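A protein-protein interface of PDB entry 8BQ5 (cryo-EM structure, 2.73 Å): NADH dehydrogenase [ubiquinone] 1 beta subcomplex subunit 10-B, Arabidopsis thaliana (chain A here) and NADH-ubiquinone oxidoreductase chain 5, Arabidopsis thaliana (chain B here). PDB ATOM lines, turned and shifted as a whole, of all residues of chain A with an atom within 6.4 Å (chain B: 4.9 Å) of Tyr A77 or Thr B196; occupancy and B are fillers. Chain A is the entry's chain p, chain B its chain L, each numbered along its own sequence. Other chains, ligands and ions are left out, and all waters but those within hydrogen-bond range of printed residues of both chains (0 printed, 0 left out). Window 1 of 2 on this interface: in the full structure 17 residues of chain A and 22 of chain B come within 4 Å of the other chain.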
ATOM      1  N   ALA A  48       9.861  -7.183 -19.679  1.00  0.00           N
ATOM      2  CA  ALA A  48      11.270  -6.867 -19.884  1.00  0.00           C
ATOM      3  C   ALA A  48      12.176  -7.972 -19.361  1.00  0.00           C
ATOM      4  O   ALA A  48      13.231  -8.238 -19.948  1.00  0.00           O
ATOM      5  CB  ALA A  48      11.610  -5.540 -19.210  1.00  0.00           C
ATOM      6  N   LYS A  49      11.788  -8.619 -18.260  1.00  0.00           N
ATOM      7  CA  LYS A  49      12.615  -9.678 -17.691  1.00  0.00           C
ATOM      8  C   LYS A  49      12.721 -10.868 -18.636  1.00  0.00           C
ATOM      9  O   LYS A  49      13.765 -11.528 -18.697  1.00  0.00           O
ATOM     10  CB  LYS A  49      12.053 -10.110 -16.338  1.00  0.00           C
ATOM     11  CG  LYS A  49      12.338  -9.126 -15.218  1.00  0.00           C
ATOM     12  CD  LYS A  49      11.513  -9.422 -13.978  1.00  0.00           C
ATOM     13  CE  LYS A  49      12.230 -10.375 -13.033  1.00  0.00           C
ATOM     14  NZ  LYS A  49      12.367 -11.750 -13.589  1.00  0.00           N
ATOM     15  N   LEU A  51      12.452 -10.519 -21.948  1.00  0.00           N
ATOM     16  CA  LEU A  51      13.323  -9.976 -22.985  1.00  0.00           C
ATOM     17  C   LEU A  51      14.777  -9.941 -22.533  1.00  0.00           C
ATOM     18  O   LEU A  51      15.688 -10.009 -23.365  1.00  0.00           O
ATOM     19  CB  LEU A  51      12.854  -8.575 -23.377  1.00  0.00           C
ATOM     20  CG  LEU A  51      11.607  -8.481 -24.260  1.00  0.00           C
ATOM     21  CD1 LEU A  51      11.263  -7.033 -24.552  1.00  0.00           C
ATOM     22  CD2 LEU A  51      11.798  -9.253 -25.554  1.00  0.00           C
ATOM     23  N   ARG A  52      15.017  -9.823 -21.224  1.00  0.00           N
ATOM     24  CA  ARG A  52      16.384  -9.847 -20.714  1.00  0.00           C
ATOM     25  C   ARG A  52      16.993 -11.236 -20.843  1.00  0.00           C
ATOM     26  O   ARG A  52      18.194 -11.378 -21.102  1.00  0.00           O
ATOM     27  CB  ARG A  52      16.405  -9.380 -19.259  1.00  0.00           C
ATOM     28  CG  ARG A  52      17.765  -9.460 -18.588  1.00  0.00           C
ATOM     29  CD  ARG A  52      17.770  -8.686 -17.284  1.00  0.00           C
ATOM     30  NE  ARG A  52      16.907  -9.310 -16.289  1.00  0.00           N
ATOM     31  CZ  ARG A  52      16.449  -8.699 -15.205  1.00  0.00           C
ATOM     32  NH1 ARG A  52      16.767  -7.445 -14.932  1.00  0.00           N
ATOM     33  NH2 ARG A  52      15.651  -9.363 -14.375  1.00  0.00           N
ATOM     34  N   GLU A  53      16.177 -12.276 -20.662  1.00  0.00           N
ATOM     35  CA  GLU A  53      16.670 -13.644 -20.782  1.00  0.00           C
ATOM     36  C   GLU A  53      17.088 -13.966 -22.212  1.00  0.00           C
ATOM     37  O   GLU A  53      18.073 -14.680 -22.429  1.00  0.00           O
ATOM     38  CB  GLU A  53      15.604 -14.628 -20.297  1.00  0.00           C
ATOM     39  CG  GLU A  53      16.165 -15.954 -19.808  1.00  0.00           C
ATOM     40  CD  GLU A  53      16.522 -15.938 -18.334  1.00  0.00           C
ATOM     41  OE1 GLU A  53      17.712 -16.129 -18.010  1.00  0.00           O
ATOM     42  OE2 GLU A  53      15.613 -15.745 -17.497  1.00  0.00           O
ATOM     43  N   VAL A  55      18.311 -11.846 -24.444  1.00  0.00           N
ATOM     44  CA  VAL A  55      19.595 -11.183 -24.661  1.00  0.00           C
ATOM     45  C   VAL A  55      20.718 -11.990 -24.026  1.00  0.00           C
ATOM     46  O   VAL A  55      21.790 -12.172 -24.613  1.00  0.00           O
ATOM     47  CB  VAL A  55      19.552  -9.748 -24.103  1.00  0.00           C
ATOM     48  CG1 VAL A  55      20.941  -9.136 -24.090  1.00  0.00           C
ATOM     49  CG2 VAL A  55      18.586  -8.893 -24.900  1.00  0.00           C
ATOM     50  N   LYS A  56      20.479 -12.486 -22.811  1.00  0.00           N
ATOM     51  CA  LYS A  56      21.479 -13.248 -22.074  1.00  0.00           C
ATOM     52  C   LYS A  56      21.954 -14.460 -22.866  1.00  0.00           C
ATOM     53  O   LYS A  56      23.158 -14.684 -23.030  1.00  0.00           O
ATOM     54  CB  LYS A  56      20.891 -13.683 -20.730  1.00  0.00           C
ATOM     55  CG  LYS A  56      21.834 -14.462 -19.837  1.00  0.00           C
ATOM     56  CD  LYS A  56      21.074 -15.122 -18.693  1.00  0.00           C
ATOM     57  CE  LYS A  56      20.624 -14.102 -17.657  1.00  0.00           C
ATOM     58  NZ  LYS A  56      19.213 -13.670 -17.854  1.00  0.00           N
ATOM     59  N   TYR A  59      23.793 -13.609 -26.196  1.00  0.00           N
ATOM     60  CA  TYR A  59      25.199 -13.324 -25.934  1.00  0.00           C
ATOM     61  C   TYR A  59      25.985 -14.610 -25.708  1.00  0.00           C
ATOM     62  O   TYR A  59      27.123 -14.753 -26.168  1.00  0.00           O
ATOM     63  CB  TYR A  59      25.319 -12.396 -24.721  1.00  0.00           C
ATOM     64  CG  TYR A  59      26.724 -11.924 -24.418  1.00  0.00           C
ATOM     65  CD1 TYR A  59      27.232 -10.775 -25.004  1.00  0.00           C
ATOM     66  CD2 TYR A  59      27.539 -12.625 -23.540  1.00  0.00           C
ATOM     67  CE1 TYR A  59      28.506 -10.339 -24.728  1.00  0.00           C
ATOM     68  CE2 TYR A  59      28.819 -12.198 -23.259  1.00  0.00           C
ATOM     69  CZ  TYR A  59      29.297 -11.052 -23.858  1.00  0.00           C
ATOM     70  OH  TYR A  59      30.569 -10.614 -23.588  1.00  0.00           O
ATOM     71  N   HIS A  72      19.016  -6.759 -32.520  1.00  0.00           N
ATOM     72  CA  HIS A  72      17.550  -6.553 -32.388  1.00  0.00           C
ATOM     73  C   HIS A  72      17.083  -6.811 -30.950  1.00  0.00           C
ATOM     74  O   HIS A  72      16.303  -5.992 -30.448  1.00  0.00           O
ATOM     75  CB  HIS A  72      16.810  -7.436 -33.410  1.00  0.00           C
ATOM     76  CG  HIS A  72      16.914  -8.903 -33.150  1.00  0.00           C
ATOM     77  ND1 HIS A  72      15.809  -9.674 -32.843  1.00  0.00           N
ATOM     78  CD2 HIS A  72      17.975  -9.739 -33.130  1.00  0.00           C
ATOM     79  CE1 HIS A  72      16.186 -10.923 -32.660  1.00  0.00           C
ATOM     80  NE2 HIS A  72      17.510 -10.988 -32.822  1.00  0.00           N
ATOM     81  N   LEU A  73      17.527  -7.905 -30.327  1.00  0.00           N
ATOM     82  CA  LEU A  73      17.086  -8.273 -28.956  1.00  0.00           C
ATOM     83  C   LEU A  73      17.554  -7.196 -27.975  1.00  0.00           C
ATOM     84  O   LEU A  73      16.770  -6.862 -27.070  1.00  0.00           O
ATOM     85  CB  LEU A  73      17.673  -9.644 -28.608  1.00  0.00           C
ATOM     86  CG  LEU A  73      16.923 -10.837 -29.190  1.00  0.00           C
ATOM     87  CD1 LEU A  73      17.576 -12.143 -28.780  1.00  0.00           C
ATOM     88  CD2 LEU A  73      15.461 -10.814 -28.778  1.00  0.00           C
ATOM     89  N   VAL A  74      18.772  -6.680 -28.152  1.00  0.00           N
ATOM     90  CA  VAL A  74      19.300  -5.595 -27.275  1.00  0.00           C
ATOM     91  C   VAL A  74      18.360  -4.393 -27.395  1.00  0.00           C
ATOM     92  O   VAL A  74      17.868  -3.951 -26.349  1.00  0.00           O
ATOM     93  CB  VAL A  74      20.764  -5.265 -27.622  1.00  0.00           C
ATOM     94  CG1 VAL A  74      21.238  -3.949 -27.037  1.00  0.00           C
ATOM     95  CG2 VAL A  74      21.698  -6.395 -27.225  1.00  0.00           C
ATOM     96  N   GLN A  75      18.078  -3.928 -28.613  1.00  0.00           N
ATOM     97  CA  GLN A  75      17.146  -2.792 -28.855  1.00  0.00           C
ATOM     98  C   GLN A  75      15.799  -3.021 -28.152  1.00  0.00           C
ATOM     99  O   GLN A  75      15.355  -2.107 -27.449  1.00  0.00           O
ATOM    100  CB  GLN A  75      16.948  -2.629 -30.359  1.00  0.00           C
ATOM    101  CG  GLN A  75      15.865  -1.639 -30.755  1.00  0.00           C
ATOM    102  CD  GLN A  75      15.653  -1.633 -32.249  1.00  0.00           C
ATOM    103  OE1 GLN A  75      15.948  -0.656 -32.932  1.00  0.00           O
ATOM    104  NE2 GLN A  75      15.141  -2.736 -32.771  1.00  0.00           N
ATOM    105  N   GLN A  76      15.172  -4.182 -28.352  1.00  0.00           N
ATOM    106  CA  GLN A  76      13.893  -4.471 -27.712  1.00  0.00           C
ATOM    107  C   GLN A  76      14.008  -4.390 -26.197  1.00  0.00           C
ATOM    108  O   GLN A  76      13.158  -3.792 -25.528  1.00  0.00           O
ATOM    109  CB  GLN A  76      13.398  -5.855 -28.130  1.00  0.00           C
ATOM    110  CG  GLN A  76      12.500  -5.864 -29.346  1.00  0.00           C
ATOM    111  CD  GLN A  76      12.265  -7.264 -29.866  1.00  0.00           C
ATOM    112  OE1 GLN A  76      11.673  -8.099 -29.185  1.00  0.00           O
ATOM    113  NE2 GLN A  76      12.725  -7.529 -31.083  1.00  0.00           N
ATOM    114  N   TYR A  77      15.059  -4.994 -25.636  1.00  0.00           N
ATOM    115  CA  TYR A  77      15.193  -5.039 -24.185  1.00  0.00           C
ATOM    116  C   TYR A  77      15.451  -3.652 -23.610  1.00  0.00           C
ATOM    117  O   TYR A  77      14.894  -3.293 -22.567  1.00  0.00           O
ATOM    118  CB  TYR A  77      16.310  -5.999 -23.786  1.00  0.00           C
ATOM    119  CG  TYR A  77      16.825  -5.753 -22.390  1.00  0.00           C
ATOM    120  CD1 TYR A  77      18.076  -5.193 -22.178  1.00  0.00           C
ATOM    121  CD2 TYR A  77      16.050  -6.066 -21.282  1.00  0.00           C
ATOM    122  CE1 TYR A  77      18.544  -4.961 -20.904  1.00  0.00           C
ATOM    123  CE2 TYR A  77      16.509  -5.841 -20.006  1.00  0.00           C
ATOM    124  CZ  TYR A  77      17.754  -5.284 -19.822  1.00  0.00           C
ATOM    125  OH  TYR A  77      18.215  -5.056 -18.548  1.00  0.00           O
ATOM    126  N   LEU A  78      16.300  -2.862 -24.269  1.00  0.00           N
ATOM    127  CA  LEU A  78      16.566  -1.516 -23.777  1.00  0.00           C
ATOM    128  C   LEU A  78      15.321  -0.644 -23.840  1.00  0.00           C
ATOM    129  O   LEU A  78      15.082   0.153 -22.927  1.00  0.00           O
ATOM    130  CB  LEU A  78      17.706  -0.872 -24.561  1.00  0.00           C
ATOM    131  CG  LEU A  78      19.107  -1.353 -24.187  1.00  0.00           C
ATOM    132  CD1 LEU A  78      20.108  -0.940 -25.248  1.00  0.00           C
ATOM    133  CD2 LEU A  78      19.515  -0.827 -22.825  1.00  0.00           C
ATOM    134  N   ASP A  79      14.520  -0.781 -24.898  1.00  0.00           N
ATOM    135  CA  ASP A  79      13.295   0.004 -25.008  1.00  0.00           C
ATOM    136  C   ASP A  79      12.311  -0.354 -23.902  1.00  0.00           C
ATOM    137  O   ASP A  79      11.601   0.515 -23.384  1.00  0.00           O
ATOM    138  CB  ASP A  79      12.659  -0.203 -26.383  1.00  0.00           C
ATOM    139  CG  ASP A  79      13.252   0.704 -27.442  1.00  0.00           C
ATOM    140  OD1 ASP A  79      13.308   1.931 -27.215  1.00  0.00           O
ATOM    141  OD2 ASP A  79      13.655   0.192 -28.507  1.00  0.00           O
ATOM    142  N   SER A  80      12.250  -1.634 -23.530  1.00  0.00           N
ATOM    143  CA  SER A  80      11.304  -2.060 -22.503  1.00  0.00           C
ATOM    144  C   SER A  80      11.705  -1.562 -21.120  1.00  0.00           C
ATOM    145  O   SER A  80      10.836  -1.313 -20.278  1.00  0.00           O
ATOM    146  CB  SER A  80      11.187  -3.582 -22.498  1.00  0.00           C
ATOM    147  OG  SER A  80      12.347  -4.170 -21.940  1.00  0.00           O
ATOM    148  N   THR A  81      13.006  -1.419 -20.860  1.00  0.00           N
ATOM    149  CA  THR A  81      13.455  -1.008 -19.536  1.00  0.00           C
ATOM    150  C   THR A  81      13.310   0.488 -19.299  1.00  0.00           C
ATOM    151  O   THR A  81      13.382   0.927 -18.147  1.00  0.00           O
ATOM    152  CB  THR A  81      14.909  -1.420 -19.310  1.00  0.00           C
ATOM    153  OG1 THR A  81      15.727  -0.911 -20.369  1.00  0.00           O
ATOM    154  CG2 THR A  81      15.019  -2.924 -19.269  1.00  0.00           C
ATOM    155  N   ARG A  82      13.118   1.277 -20.351  1.00  0.00           N
ATOM    156  CA  ARG A  82      12.812   2.690 -20.192  1.00  0.00           C
ATOM    157  C   ARG A  82      11.327   2.826 -19.883  1.00  0.00           C
ATOM    158  O   ARG A  82      10.486   2.281 -20.605  1.00  0.00           O
ATOM    159  CB  ARG A  82      13.177   3.466 -21.456  1.00  0.00           C
ATOM    160  CG  ARG A  82      14.473   3.012 -22.097  1.00  0.00           C
ATOM    161  CD  ARG A  82      15.687   3.746 -21.555  1.00  0.00           C
ATOM    162  NE  ARG A  82      15.414   5.150 -21.276  1.00  0.00           N
ATOM    163  CZ  ARG A  82      16.322   6.011 -20.840  1.00  0.00           C
ATOM    164  NH1 ARG A  82      17.574   5.644 -20.622  1.00  0.00           N
ATOM    165  NH2 ARG A  82      15.966   7.274 -20.621  1.00  0.00           N
ATOM    166  N   PHE B 189      21.408  -0.149 -16.812  1.00  0.00           N
ATOM    167  CA  PHE B 189      20.971  -1.304 -17.586  1.00  0.00           C
ATOM    168  C   PHE B 189      19.782  -2.041 -16.978  1.00  0.00           C
ATOM    169  O   PHE B 189      19.226  -2.926 -17.638  1.00  0.00           O
ATOM    170  CB  PHE B 189      22.132  -2.294 -17.758  1.00  0.00           C
ATOM    171  CG  PHE B 189      23.344  -1.706 -18.429  1.00  0.00           C
ATOM    172  CD1 PHE B 189      23.369  -1.511 -19.800  1.00  0.00           C
ATOM    173  CD2 PHE B 189      24.464  -1.362 -17.689  1.00  0.00           C
ATOM    174  CE1 PHE B 189      24.483  -0.977 -20.418  1.00  0.00           C
ATOM    175  CE2 PHE B 189      25.579  -0.828 -18.303  1.00  0.00           C
ATOM    176  CZ  PHE B 189      25.589  -0.636 -19.670  1.00  0.00           C
ATOM    177  N   GLN B 190      19.384  -1.707 -15.750  1.00  0.00           N
ATOM    178  CA  GLN B 190      18.327  -2.418 -15.025  1.00  0.00           C
ATOM    179  C   GLN B 190      18.628  -3.909 -14.898  1.00  0.00           C
ATOM    180  O   GLN B 190      17.717  -4.740 -14.909  1.00  0.00           O
ATOM    181  CB  GLN B 190      16.952  -2.188 -15.659  1.00  0.00           C
ATOM    182  CG  GLN B 190      16.432  -0.770 -15.472  1.00  0.00           C
ATOM    183  CD  GLN B 190      16.214  -0.415 -14.012  1.00  0.00           C
ATOM    184  OE1 GLN B 190      15.304  -0.930 -13.362  1.00  0.00           O
ATOM    185  NE2 GLN B 190      17.055   0.467 -13.487  1.00  0.00           N
ATOM    186  N   THR B 191      19.907  -4.252 -14.765  1.00  0.00           N
ATOM    187  CA  THR B 191      20.322  -5.623 -14.510  1.00  0.00           C
ATOM    188  C   THR B 191      21.752  -5.611 -13.993  1.00  0.00           C
ATOM    189  O   THR B 191      22.524  -4.689 -14.268  1.00  0.00           O
ATOM    190  CB  THR B 191      20.219  -6.497 -15.765  1.00  0.00           C
ATOM    191  OG1 THR B 191      20.469  -7.864 -15.419  1.00  0.00           O
ATOM    192  CG2 THR B 191      21.231  -6.055 -16.808  1.00  0.00           C
ATOM    193  N   ASP B 193      23.364  -8.779 -14.269  1.00  0.00           N
ATOM    194  CA  ASP B 193      23.919  -9.953 -14.995  1.00  0.00           C
ATOM    195  C   ASP B 193      25.040  -9.510 -15.930  1.00  0.00           C
ATOM    196  O   ASP B 193      24.828  -8.560 -16.684  1.00  0.00           O
ATOM    197  CB  ASP B 193      22.864 -10.693 -15.814  1.00  0.00           C
ATOM    198  CG  ASP B 193      23.357 -12.029 -16.338  1.00  0.00           C
ATOM    199  OD1 ASP B 193      23.402 -12.989 -15.547  1.00  0.00           O
ATOM    200  OD2 ASP B 193      23.707 -12.096 -17.527  1.00  0.00           O
ATOM    201  N   PHE B 194      26.172 -10.205 -15.884  1.00  0.00           N
ATOM    202  CA  PHE B 194      27.339  -9.842 -16.722  1.00  0.00           C
ATOM    203  C   PHE B 194      26.982  -9.986 -18.203  1.00  0.00           C
ATOM    204  O   PHE B 194      27.212  -9.019 -18.935  1.00  0.00           O
ATOM    205  CB  PHE B 194      28.538 -10.729 -16.383  1.00  0.00           C
ATOM    206  CG  PHE B 194      29.324 -10.323 -15.164  1.00  0.00           C
ATOM    207  CD1 PHE B 194      29.491  -8.988 -14.836  1.00  0.00           C
ATOM    208  CD2 PHE B 194      29.918 -11.277 -14.354  1.00  0.00           C
ATOM    209  CE1 PHE B 194      30.220  -8.620 -13.719  1.00  0.00           C
ATOM    210  CE2 PHE B 194      30.646 -10.908 -13.236  1.00  0.00           C
ATOM    211  CZ  PHE B 194      30.794  -9.579 -12.920  1.00  0.00           C
ATOM    212  N   SER B 195      26.399 -11.121 -18.619  1.00  0.00           N
ATOM    213  CA  SER B 195      26.163 -11.343 -20.043  1.00  0.00           C
ATOM    214  C   SER B 195      25.251 -10.277 -20.633  1.00  0.00           C
ATOM    215  O   SER B 195      25.488  -9.796 -21.747  1.00  0.00           O
ATOM    216  CB  SER B 195      25.564 -12.730 -20.271  1.00  0.00           C
ATOM    217  OG  SER B 195      26.151 -13.690 -19.415  1.00  0.00           O
ATOM    218  N   THR B 196      24.194  -9.908 -19.909  1.00  0.00           N
ATOM    219  CA  THR B 196      23.257  -8.909 -20.409  1.00  0.00           C
ATOM    220  C   THR B 196      23.920  -7.544 -20.542  1.00  0.00           C
ATOM    221  O   THR B 196      23.720  -6.838 -21.537  1.00  0.00           O
ATOM    222  CB  THR B 196      22.042  -8.830 -19.487  1.00  0.00           C
ATOM    223  OG1 THR B 196      21.445 -10.126 -19.374  1.00  0.00           O
ATOM    224  CG2 THR B 196      21.020  -7.846 -20.032  1.00  0.00           C
ATOM    225  N   ILE B 197      24.711  -7.155 -19.540  1.00  0.00           N
ATOM    226  CA  ILE B 197      25.369  -5.851 -19.564  1.00  0.00           C
ATOM    227  C   ILE B 197      26.394  -5.786 -20.688  1.00  0.00           C
ATOM    228  O   ILE B 197      26.472  -4.792 -21.421  1.00  0.00           O
ATOM    229  CB  ILE B 197      26.007  -5.557 -18.194  1.00  0.00           C
ATOM    230  CG1 ILE B 197      24.929  -5.204 -17.170  1.00  0.00           C
ATOM    231  CG2 ILE B 197      27.033  -4.439 -18.303  1.00  0.00           C
ATOM    232  CD1 ILE B 197      25.400  -5.312 -15.745  1.00  0.00           C
ATOM    233  N   PHE B 198      27.198  -6.841 -20.843  1.00  0.00           N
ATOM    234  CA  PHE B 198      28.214  -6.849 -21.889  1.00  0.00           C
ATOM    235  C   PHE B 198      27.592  -6.821 -23.278  1.00  0.00           C
ATOM    236  O   PHE B 198      28.178  -6.256 -24.208  1.00  0.00           O
ATOM    237  CB  PHE B 198      29.120  -8.070 -21.733  1.00  0.00           C
ATOM    238  CG  PHE B 198      29.908  -8.076 -20.456  1.00  0.00           C
ATOM    239  CD1 PHE B 198      30.187  -6.890 -19.797  1.00  0.00           C
ATOM    240  CD2 PHE B 198      30.370  -9.262 -19.915  1.00  0.00           C
ATOM    241  CE1 PHE B 198      30.908  -6.888 -18.624  1.00  0.00           C
ATOM    242  CE2 PHE B 198      31.094  -9.265 -18.741  1.00  0.00           C
ATOM    243  CZ  PHE B 198      31.361  -8.076 -18.095  1.00  0.00           C
ATOM    244  N   ALA B 199      26.409  -7.417 -23.435  1.00  0.00           N
ATOM    245  CA  ALA B 199      25.696  -7.359 -24.702  1.00  0.00           C
ATOM    246  C   ALA B 199      25.111  -5.981 -24.979  1.00  0.00           C
ATOM    247  O   ALA B 199      24.896  -5.636 -26.146  1.00  0.00           O
ATOM    248  CB  ALA B 199      24.583  -8.406 -24.723  1.00  0.00           C
ATOM    249  N   CYS B 200      24.853  -5.188 -23.940  1.00  0.00           N
ATOM    250  CA  CYS B 200      24.185  -3.903 -24.092  1.00  0.00           C
ATOM    251  C   CYS B 200      25.121  -2.708 -23.971  1.00  0.00           C
ATOM    252  O   CYS B 200      24.686  -1.582 -24.229  1.00  0.00           O
ATOM    253  CB  CYS B 200      23.068  -3.764 -23.047  1.00  0.00           C
ATOM    254  SG  CYS B 200      21.681  -4.903 -23.248  1.00  0.00           S
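Tyr A77 touches just these residues of chain B: Phe B189, Gln B190, Thr B191, Thr B196 and Cys B200.
Of the printed residues of chain A, Thr B196 touches Arg A52 (3.8 Å), Lys A56 (3.8 Å) and Tyr A77 (3.9 Å).
Printed residues of chain A within 4 Å of Gln B190: Arg A52 and Tyr A77.
Of the printed residues of chain A, Phe B189 touches Tyr A77 (2.5 Å).
Of the printed residues of chain A, Ala B199 touches Val A55, Tyr A59 and Val A74.
The nearest printed residue of chain B that does not touch Tyr A77 is Ile B197 (6.7 Å).
The nearest residue of chain A that does not touch Thr B196 is Val A55 (4.3 Å).
The nearest printed residue of chain A that does not touch Ser B195 is Lys A56 (4.1 Å).
Arg A52 touches Thr B191 (CD to OG1, 3.4 Å).
Arg A52 touches Thr B196 (CG to OG1, 3.8 Å).
CG1 of Val A55 touches CB of Ala B199 (3.8 Å).
Lys A56 touches Asp B193 (CE to OD1, 3.7 Å).
Thr B196 touches Lys A56.
O of Ala B199 touches CG2 of Val A74, at 3.5 Å.
SG of Cys B200 touches CG1 of Val A74, at 3.9 Å.
OH of Tyr A77 touches CG2 of Thr B191 (3.6 Å).
Thr B196 touches Tyr A77.
Tyr A77 touches Cys B200.
The side-chain amino group (NZ) of Lys A56 is in salt-bridge range of the side-chain carboxylate (OE1) of Glu A53 (2.9 Å).
The side-chain hydroxyl of Ser A80 lies within hydrogen-bond range of the backbone carbonyl oxygen of Tyr A77 (2.8 Å).
The side-chain hydroxyl of Thr B191 sits at hydrogen-bond distance from the backbone NH of Asp B193, 3.2 Å away.
OD2 of Asp B193 is in hydrogen-bond range of N of Thr B196 (3.3 Å).
N of Ser B195 sits at hydrogen-bond distance from OD2 of Asp B193 (3.1 Å).
OG1 of Thr A81 sits close to O of Tyr A77 (3.3 Å).
Hydrophobic or aromatic side chains of chain A within 4 Å of the printed part of chain B: Val A55, Tyr A59, Val A74 and Tyr A77.
Of the 11 printed residues of chain B, 9 touch a printed residue of chain A.
Hydrophobic or aromatic side chains of chain B within 4 Å of the printed part of chain A: Phe B198 and Ala B199.
Along chain B the printed residues that touch a printed residue of chain A span positions 189 to 200.
Among the printed residues, 16 pairs touch across the chains.
The backbone carbonyl oxygen of Phe B189 sits at hydrogen-bond distance from the side-chain hydroxyl of Tyr A77 (2.5 Å).
The guanidinium group (NH1) of Arg A52 lies within hydrogen-bond range of the backbone carbonyl oxygen (O) of Gln B190, 2.9 Å away.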
